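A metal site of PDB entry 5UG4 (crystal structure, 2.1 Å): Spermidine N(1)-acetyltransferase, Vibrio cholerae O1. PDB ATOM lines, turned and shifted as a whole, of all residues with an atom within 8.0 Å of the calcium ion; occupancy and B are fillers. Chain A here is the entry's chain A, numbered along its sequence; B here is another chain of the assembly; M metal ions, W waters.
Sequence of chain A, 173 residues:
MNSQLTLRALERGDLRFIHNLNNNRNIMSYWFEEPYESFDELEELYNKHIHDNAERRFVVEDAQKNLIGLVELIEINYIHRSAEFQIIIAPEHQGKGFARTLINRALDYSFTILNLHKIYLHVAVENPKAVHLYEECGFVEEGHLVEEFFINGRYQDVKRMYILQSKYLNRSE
N of Glu 41 sits at hydrogen-bond distance from OG of Ser 38, 3.1 Å away.
O of Asn 53 of chain B sits at hydrogen-bond distance from OH of Tyr 78 of chain B, 2.6 Å away.
The side-chain carboxylate of Glu 41 lies close to a ring nitrogen (ND1) of His 51 of chain B (2.9 Å).
OE2 of Glu 34 binds the calcium ion, at 2.3 Å.
The calcium ion is bound by the side-chain carboxylate (OE2) of Glu 41 (2.4 Å).
Water W2 is bound to the calcium ion (2.4 Å).
OD1 of Asn 53 of chain B binds the calcium ion, 2.4 Å away.
The side-chain carboxylate (OE1) of Glu 41 binds the calcium ion (2.5 Å).
O of Pro 35 is bound to the calcium ion (2.5 Å).
The calcium ion is bound by water W1 (2.5 Å).
The calcium ion has seven donor atoms within binding distance.
Water W1 lies within hydrogen-bond range of O of Ile 50 of chain B (2.7 Å), O of Asp 52 of chain B (3.2 Å) and NH1 of Arg 56 of chain B (3.3 Å).
Four residues have an atom within 4 Å of the calcium ion: Glu 34, Pro 35, Glu 41 and Asn 53 of chain B.
The nearest printed residue that does not touch the calcium ion is His 51 of chain B (4.2 Å).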
ATOM      1  N   MET A  28      20.550  13.675 -30.052  1.00  0.00           N
ATOM      2  CA  MET A  28      20.356  12.688 -28.980  1.00  0.00           C
ATOM      3  C   MET A  28      20.301  13.400 -27.618  1.00  0.00           C
ATOM      4  O   MET A  28      21.202  14.166 -27.278  1.00  0.00           O
ATOM      5  CB  MET A  28      21.453  11.632 -28.932  1.00  0.00           C
ATOM      6  CG  MET A  28      21.209  10.537 -27.886  1.00  0.00           C
ATOM      7  SD  MET A  28      19.694   9.571 -28.146  1.00  0.00           S
ATOM      8  CE  MET A  28      20.150   8.685 -29.588  1.00  0.00           C
ATOM      9  N   SER A  29      19.239  13.152 -26.891  1.00  0.00           N
ATOM     10  CA  SER A  29      19.049  13.711 -25.560  1.00  0.00           C
ATOM     11  C   SER A  29      19.349  12.662 -24.463  1.00  0.00           C
ATOM     12  O   SER A  29      19.312  11.452 -24.719  1.00  0.00           O
ATOM     13  CB  SER A  29      17.616  14.216 -25.408  1.00  0.00           C
ATOM     14  OG  SER A  29      17.394  15.203 -26.395  1.00  0.00           O
ATOM     15  N   GLU A  33      22.667  10.854 -17.884  1.00  0.00           N
ATOM     16  CA  GLU A  33      23.623  10.170 -18.764  1.00  0.00           C
ATOM     17  C   GLU A  33      23.019   9.041 -19.565  1.00  0.00           C
ATOM     18  O   GLU A  33      23.734   8.444 -20.339  1.00  0.00           O
ATOM     19  CB  GLU A  33      24.876   9.615 -18.013  1.00  0.00           C
ATOM     20  CG  GLU A  33      25.456  10.510 -16.948  1.00  0.00           C
ATOM     21  CD  GLU A  33      26.591  11.371 -17.432  1.00  0.00           C
ATOM     22  OE1 GLU A  33      26.726  11.551 -18.688  1.00  0.00           O
ATOM     23  OE2 GLU A  33      27.362  11.884 -16.574  1.00  0.00           O
ATOM     24  N   GLU A  34      21.730   8.706 -19.401  1.00  0.00           N
ATOM     25  CA  GLU A  34      21.098   7.673 -20.212  1.00  0.00           C
ATOM     26  C   GLU A  34      20.541   8.383 -21.469  1.00  0.00           C
ATOM     27  O   GLU A  34      19.747   9.321 -21.351  1.00  0.00           O
ATOM     28  CB  GLU A  34      20.007   6.914 -19.435  1.00  0.00           C
ATOM     29  CG  GLU A  34      19.108   5.997 -20.356  1.00  0.00           C
ATOM     30  CD  GLU A  34      19.831   4.820 -21.027  1.00  0.00           C
ATOM     31  OE1 GLU A  34      20.813   4.327 -20.392  1.00  0.00           O
ATOM     32  OE2 GLU A  34      19.386   4.380 -22.151  1.00  0.00           O
ATOM     33  N   PRO A  35      20.926   7.925 -22.666  1.00  0.00           N
ATOM     34  CA  PRO A  35      20.298   8.441 -23.872  1.00  0.00           C
ATOM     35  C   PRO A  35      18.876   7.993 -23.978  1.00  0.00           C
ATOM     36  O   PRO A  35      18.554   6.883 -23.546  1.00  0.00           O
ATOM     37  CB  PRO A  35      21.160   7.804 -25.016  1.00  0.00           C
ATOM     38  CG  PRO A  35      21.670   6.500 -24.434  1.00  0.00           C
ATOM     39  CD  PRO A  35      21.959   6.884 -22.964  1.00  0.00           C
ATOM     40  N   TYR A  36      17.995   8.843 -24.491  1.00  0.00           N
ATOM     41  CA  TYR A  36      16.626   8.419 -24.687  1.00  0.00           C
ATOM     42  C   TYR A  36      16.098   9.109 -25.898  1.00  0.00           C
ATOM     43  O   TYR A  36      16.544  10.224 -26.211  1.00  0.00           O
ATOM     44  CB  TYR A  36      15.759   8.780 -23.469  1.00  0.00           C
ATOM     45  CG  TYR A  36      15.514  10.228 -23.300  1.00  0.00           C
ATOM     46  CD1 TYR A  36      16.393  11.024 -22.607  1.00  0.00           C
ATOM     47  CD2 TYR A  36      14.410  10.817 -23.894  1.00  0.00           C
ATOM     48  CE1 TYR A  36      16.192  12.396 -22.498  1.00  0.00           C
ATOM     49  CE2 TYR A  36      14.192  12.185 -23.780  1.00  0.00           C
ATOM     50  CZ  TYR A  36      15.090  12.950 -23.088  1.00  0.00           C
ATOM     51  OH  TYR A  36      14.850  14.266 -23.019  1.00  0.00           O
ATOM     52  N   GLU A  37      15.127   8.471 -26.536  1.00  0.00           N
ATOM     53  CA  GLU A  37      14.400   9.015 -27.706  1.00  0.00           C
ATOM     54  C   GLU A  37      12.910   9.140 -27.550  1.00  0.00           C
ATOM     55  O   GLU A  37      12.282   9.902 -28.229  1.00  0.00           O
ATOM     56  CB  GLU A  37      14.674   8.095 -28.910  1.00  0.00           C
ATOM     57  CG  GLU A  37      16.145   8.073 -29.256  1.00  0.00           C
ATOM     58  CD  GLU A  37      16.592   6.702 -29.768  1.00  0.00           C
ATOM     59  OE1 GLU A  37      15.830   5.705 -29.679  1.00  0.00           O
ATOM     60  OE2 GLU A  37      17.707   6.630 -30.236  1.00  0.00           O
ATOM     61  N   SER A  38      12.317   8.325 -26.695  1.00  0.00           N
ATOM     62  CA  SER A  38      10.839   8.289 -26.580  1.00  0.00           C
ATOM     63  C   SER A  38      10.379   8.941 -25.326  1.00  0.00           C
ATOM     64  O   SER A  38      11.121   8.994 -24.349  1.00  0.00           O
ATOM     65  CB  SER A  38      10.368   6.821 -26.534  1.00  0.00           C
ATOM     66  OG  SER A  38      10.930   6.155 -25.431  1.00  0.00           O
ATOM     67  N   GLU A  41      10.483   6.361 -22.409  1.00  0.00           N
ATOM     68  CA  GLU A  41      11.728   6.177 -21.693  1.00  0.00           C
ATOM     69  C   GLU A  41      12.063   7.457 -20.836  1.00  0.00           C
ATOM     70  O   GLU A  41      12.524   7.341 -19.684  1.00  0.00           O
ATOM     71  CB  GLU A  41      12.949   5.839 -22.562  1.00  0.00           C
ATOM     72  CG  GLU A  41      14.129   5.460 -21.666  1.00  0.00           C
ATOM     73  CD  GLU A  41      15.384   5.049 -22.396  1.00  0.00           C
ATOM     74  OE1 GLU A  41      16.325   4.483 -21.702  1.00  0.00           O
ATOM     75  OE2 GLU A  41      15.456   5.218 -23.662  1.00  0.00           O
ATOM     76  N   LEU A  42      11.725   8.620 -21.372  1.00  0.00           N
ATOM     77  CA  LEU A  42      11.899   9.856 -20.600  1.00  0.00           C
ATOM     78  C   LEU A  42      11.132   9.768 -19.261  1.00  0.00           C
ATOM     79  O   LEU A  42      11.672  10.001 -18.175  1.00  0.00           O
ATOM     80  CB  LEU A  42      11.475  11.062 -21.396  1.00  0.00           C
ATOM     81  CG  LEU A  42      11.490  12.404 -20.597  1.00  0.00           C
ATOM     82  CD1 LEU A  42      12.868  12.763 -20.048  1.00  0.00           C
ATOM     83  CD2 LEU A  42      10.915  13.474 -21.539  1.00  0.00           C
ATOM     84  N   LEU A  45      12.849   7.307 -16.837  1.00  0.00           N
ATOM     85  CA  LEU A  45      14.044   7.900 -16.295  1.00  0.00           C
ATOM     86  C   LEU A  45      13.725   9.017 -15.269  1.00  0.00           C
ATOM     87  O   LEU A  45      14.331   9.083 -14.246  1.00  0.00           O
ATOM     88  CB  LEU A  45      14.930   8.453 -17.410  1.00  0.00           C
ATOM     89  CG  LEU A  45      15.592   7.357 -18.263  1.00  0.00           C
ATOM     90  CD1 LEU A  45      16.112   7.958 -19.547  1.00  0.00           C
ATOM     91  CD2 LEU A  45      16.703   6.595 -17.538  1.00  0.00           C
ATOM     92  N   HIS B  49      12.242  -3.941 -21.645  1.00  0.00           N
ATOM     93  CA  HIS B  49      13.503  -3.542 -22.319  1.00  0.00           C
ATOM     94  C   HIS B  49      13.592  -2.089 -22.639  1.00  0.00           C
ATOM     95  O   HIS B  49      14.356  -1.659 -23.516  1.00  0.00           O
ATOM     96  CB  HIS B  49      13.641  -4.416 -23.631  1.00  0.00           C
ATOM     97  CG  HIS B  49      13.826  -5.843 -23.343  1.00  0.00           C
ATOM     98  ND1 HIS B  49      15.050  -6.405 -23.051  1.00  0.00           N
ATOM     99  CD2 HIS B  49      12.929  -6.867 -23.289  1.00  0.00           C
ATOM    100  CE1 HIS B  49      14.898  -7.684 -22.784  1.00  0.00           C
ATOM    101  NE2 HIS B  49      13.627  -8.004 -22.958  1.00  0.00           N
ATOM    102  N   ILE B  50      12.789  -1.289 -21.964  1.00  0.00           N
ATOM    103  CA  ILE B  50      12.684   0.106 -22.251  1.00  0.00           C
ATOM    104  C   ILE B  50      14.038   0.845 -22.204  1.00  0.00           C
ATOM    105  O   ILE B  50      14.209   1.785 -22.937  1.00  0.00           O
ATOM    106  CB  ILE B  50      11.606   0.785 -21.350  1.00  0.00           C
ATOM    107  CG1 ILE B  50      11.263   2.204 -21.768  1.00  0.00           C
ATOM    108  CG2 ILE B  50      11.978   0.908 -19.873  1.00  0.00           C
ATOM    109  CD1 ILE B  50      10.191   2.172 -22.802  1.00  0.00           C
ATOM    110  N   HIS B  51      14.970   0.420 -21.359  1.00  0.00           N
ATOM    111  CA  HIS B  51      16.267   1.077 -21.173  1.00  0.00           C
ATOM    112  C   HIS B  51      17.373   0.373 -21.944  1.00  0.00           C
ATOM    113  O   HIS B  51      18.510   0.820 -21.919  1.00  0.00           O
ATOM    114  CB  HIS B  51      16.636   1.155 -19.692  1.00  0.00           C
ATOM    115  CG  HIS B  51      15.701   2.005 -18.899  1.00  0.00           C
ATOM    116  ND1 HIS B  51      15.377   3.286 -19.283  1.00  0.00           N
ATOM    117  CD2 HIS B  51      14.963   1.727 -17.795  1.00  0.00           C
ATOM    118  CE1 HIS B  51      14.525   3.789 -18.398  1.00  0.00           C
ATOM    119  NE2 HIS B  51      14.229   2.848 -17.517  1.00  0.00           N
ATOM    120  N   ASP B  52      17.034  -0.677 -22.658  1.00  0.00           N
ATOM    121  CA  ASP B  52      18.025  -1.351 -23.463  1.00  0.00           C
ATOM    122  C   ASP B  52      18.282  -0.639 -24.791  1.00  0.00           C
ATOM    123  O   ASP B  52      17.351  -0.390 -25.582  1.00  0.00           O
ATOM    124  CB  ASP B  52      17.576  -2.802 -23.647  1.00  0.00           C
ATOM    125  CG  ASP B  52      18.709  -3.711 -24.148  1.00  0.00           C
ATOM    126  OD1 ASP B  52      19.630  -3.272 -24.895  1.00  0.00           O
ATOM    127  OD2 ASP B  52      18.594  -4.886 -23.859  1.00  0.00           O
ATOM    128  N   ASN B  53      19.541  -0.281 -25.054  1.00  0.00           N
ATOM    129  CA  ASN B  53      19.910   0.461 -26.228  1.00  0.00           C
ATOM    130  C   ASN B  53      20.415  -0.448 -27.414  1.00  0.00           C
ATOM    131  O   ASN B  53      20.800   0.060 -28.448  1.00  0.00           O
ATOM    132  CB  ASN B  53      20.974   1.525 -25.874  1.00  0.00           C
ATOM    133  CG  ASN B  53      20.412   2.554 -24.828  1.00  0.00           C
ATOM    134  OD1 ASN B  53      19.304   3.101 -24.981  1.00  0.00           O
ATOM    135  ND2 ASN B  53      21.151   2.737 -23.729  1.00  0.00           N
ATOM    136  N   ALA B  54      20.348  -1.752 -27.264  1.00  0.00           N
ATOM    137  CA  ALA B  54      20.783  -2.702 -28.311  1.00  0.00           C
ATOM    138  C   ALA B  54      19.819  -2.803 -29.490  1.00  0.00           C
ATOM    139  O   ALA B  54      20.172  -3.296 -30.599  1.00  0.00           O
ATOM    140  CB  ALA B  54      21.032  -4.074 -27.697  1.00  0.00           C
ATOM    141  N   GLU B  55      18.575  -2.336 -29.287  1.00  0.00           N
ATOM    142  CA  GLU B  55      17.603  -2.224 -30.365  1.00  0.00           C
ATOM    143  C   GLU B  55      16.858  -0.940 -30.218  1.00  0.00           C
ATOM    144  O   GLU B  55      16.539  -0.569 -29.093  1.00  0.00           O
ATOM    145  CB  GLU B  55      16.599  -3.413 -30.394  1.00  0.00           C
ATOM    146  CG  GLU B  55      17.257  -4.799 -30.241  1.00  0.00           C
ATOM    147  CD  GLU B  55      16.240  -5.967 -30.298  1.00  0.00           C
ATOM    148  OE1 GLU B  55      16.732  -7.106 -30.436  1.00  0.00           O
ATOM    149  OE2 GLU B  55      15.002  -5.806 -30.141  1.00  0.00           O
ATOM    150  N   ARG B  56      16.529  -0.316 -31.350  1.00  0.00           N
ATOM    151  CA  ARG B  56      15.858   1.000 -31.393  1.00  0.00           C
ATOM    152  C   ARG B  56      14.844   0.931 -32.498  1.00  0.00           C
ATOM    153  O   ARG B  56      15.176   0.427 -33.602  1.00  0.00           O
ATOM    154  CB  ARG B  56      16.829   2.142 -31.723  1.00  0.00           C
ATOM    155  CG  ARG B  56      17.979   2.332 -30.776  1.00  0.00           C
ATOM    156  CD  ARG B  56      17.659   2.348 -29.311  1.00  0.00           C
ATOM    157  NE  ARG B  56      16.620   3.252 -28.807  1.00  0.00           N
ATOM    158  CZ  ARG B  56      15.650   2.900 -27.949  1.00  0.00           C
ATOM    159  NH1 ARG B  56      15.527   1.635 -27.470  1.00  0.00           N
ATOM    160  NH2 ARG B  56      14.834   3.850 -27.531  1.00  0.00           N
ATOM    161  N   TYR B  78      28.083  -0.997 -30.036  1.00  0.00           N
ATOM    162  CA  TYR B  78      28.611   0.357 -29.877  1.00  0.00           C
ATOM    163  C   TYR B  78      30.138   0.392 -29.877  1.00  0.00           C
ATOM    164  O   TYR B  78      30.741   1.429 -29.654  1.00  0.00           O
ATOM    165  CB  TYR B  78      27.989   1.098 -28.669  1.00  0.00           C
ATOM    166  CG  TYR B  78      26.473   1.371 -28.776  1.00  0.00           C
ATOM    167  CD1 TYR B  78      25.521   0.384 -28.371  1.00  0.00           C
ATOM    168  CD2 TYR B  78      25.974   2.542 -29.328  1.00  0.00           C
ATOM    169  CE1 TYR B  78      24.152   0.614 -28.505  1.00  0.00           C
ATOM    170  CE2 TYR B  78      24.597   2.765 -29.454  1.00  0.00           C
ATOM    171  CZ  TYR B  78      23.697   1.794 -29.032  1.00  0.00           C
ATOM    172  OH  TYR B  78      22.342   2.051 -29.165  1.00  0.00           O
HETATM  173 CA    CA M   1      17.749   4.496 -23.705  1.00  0.00          CA
HETATM  174  O   HOH W   1      16.427   2.422 -24.364  1.00  0.00           O
HETATM  175  O   HOH W   2      17.402   5.170 -25.993  1.00  0.00           O
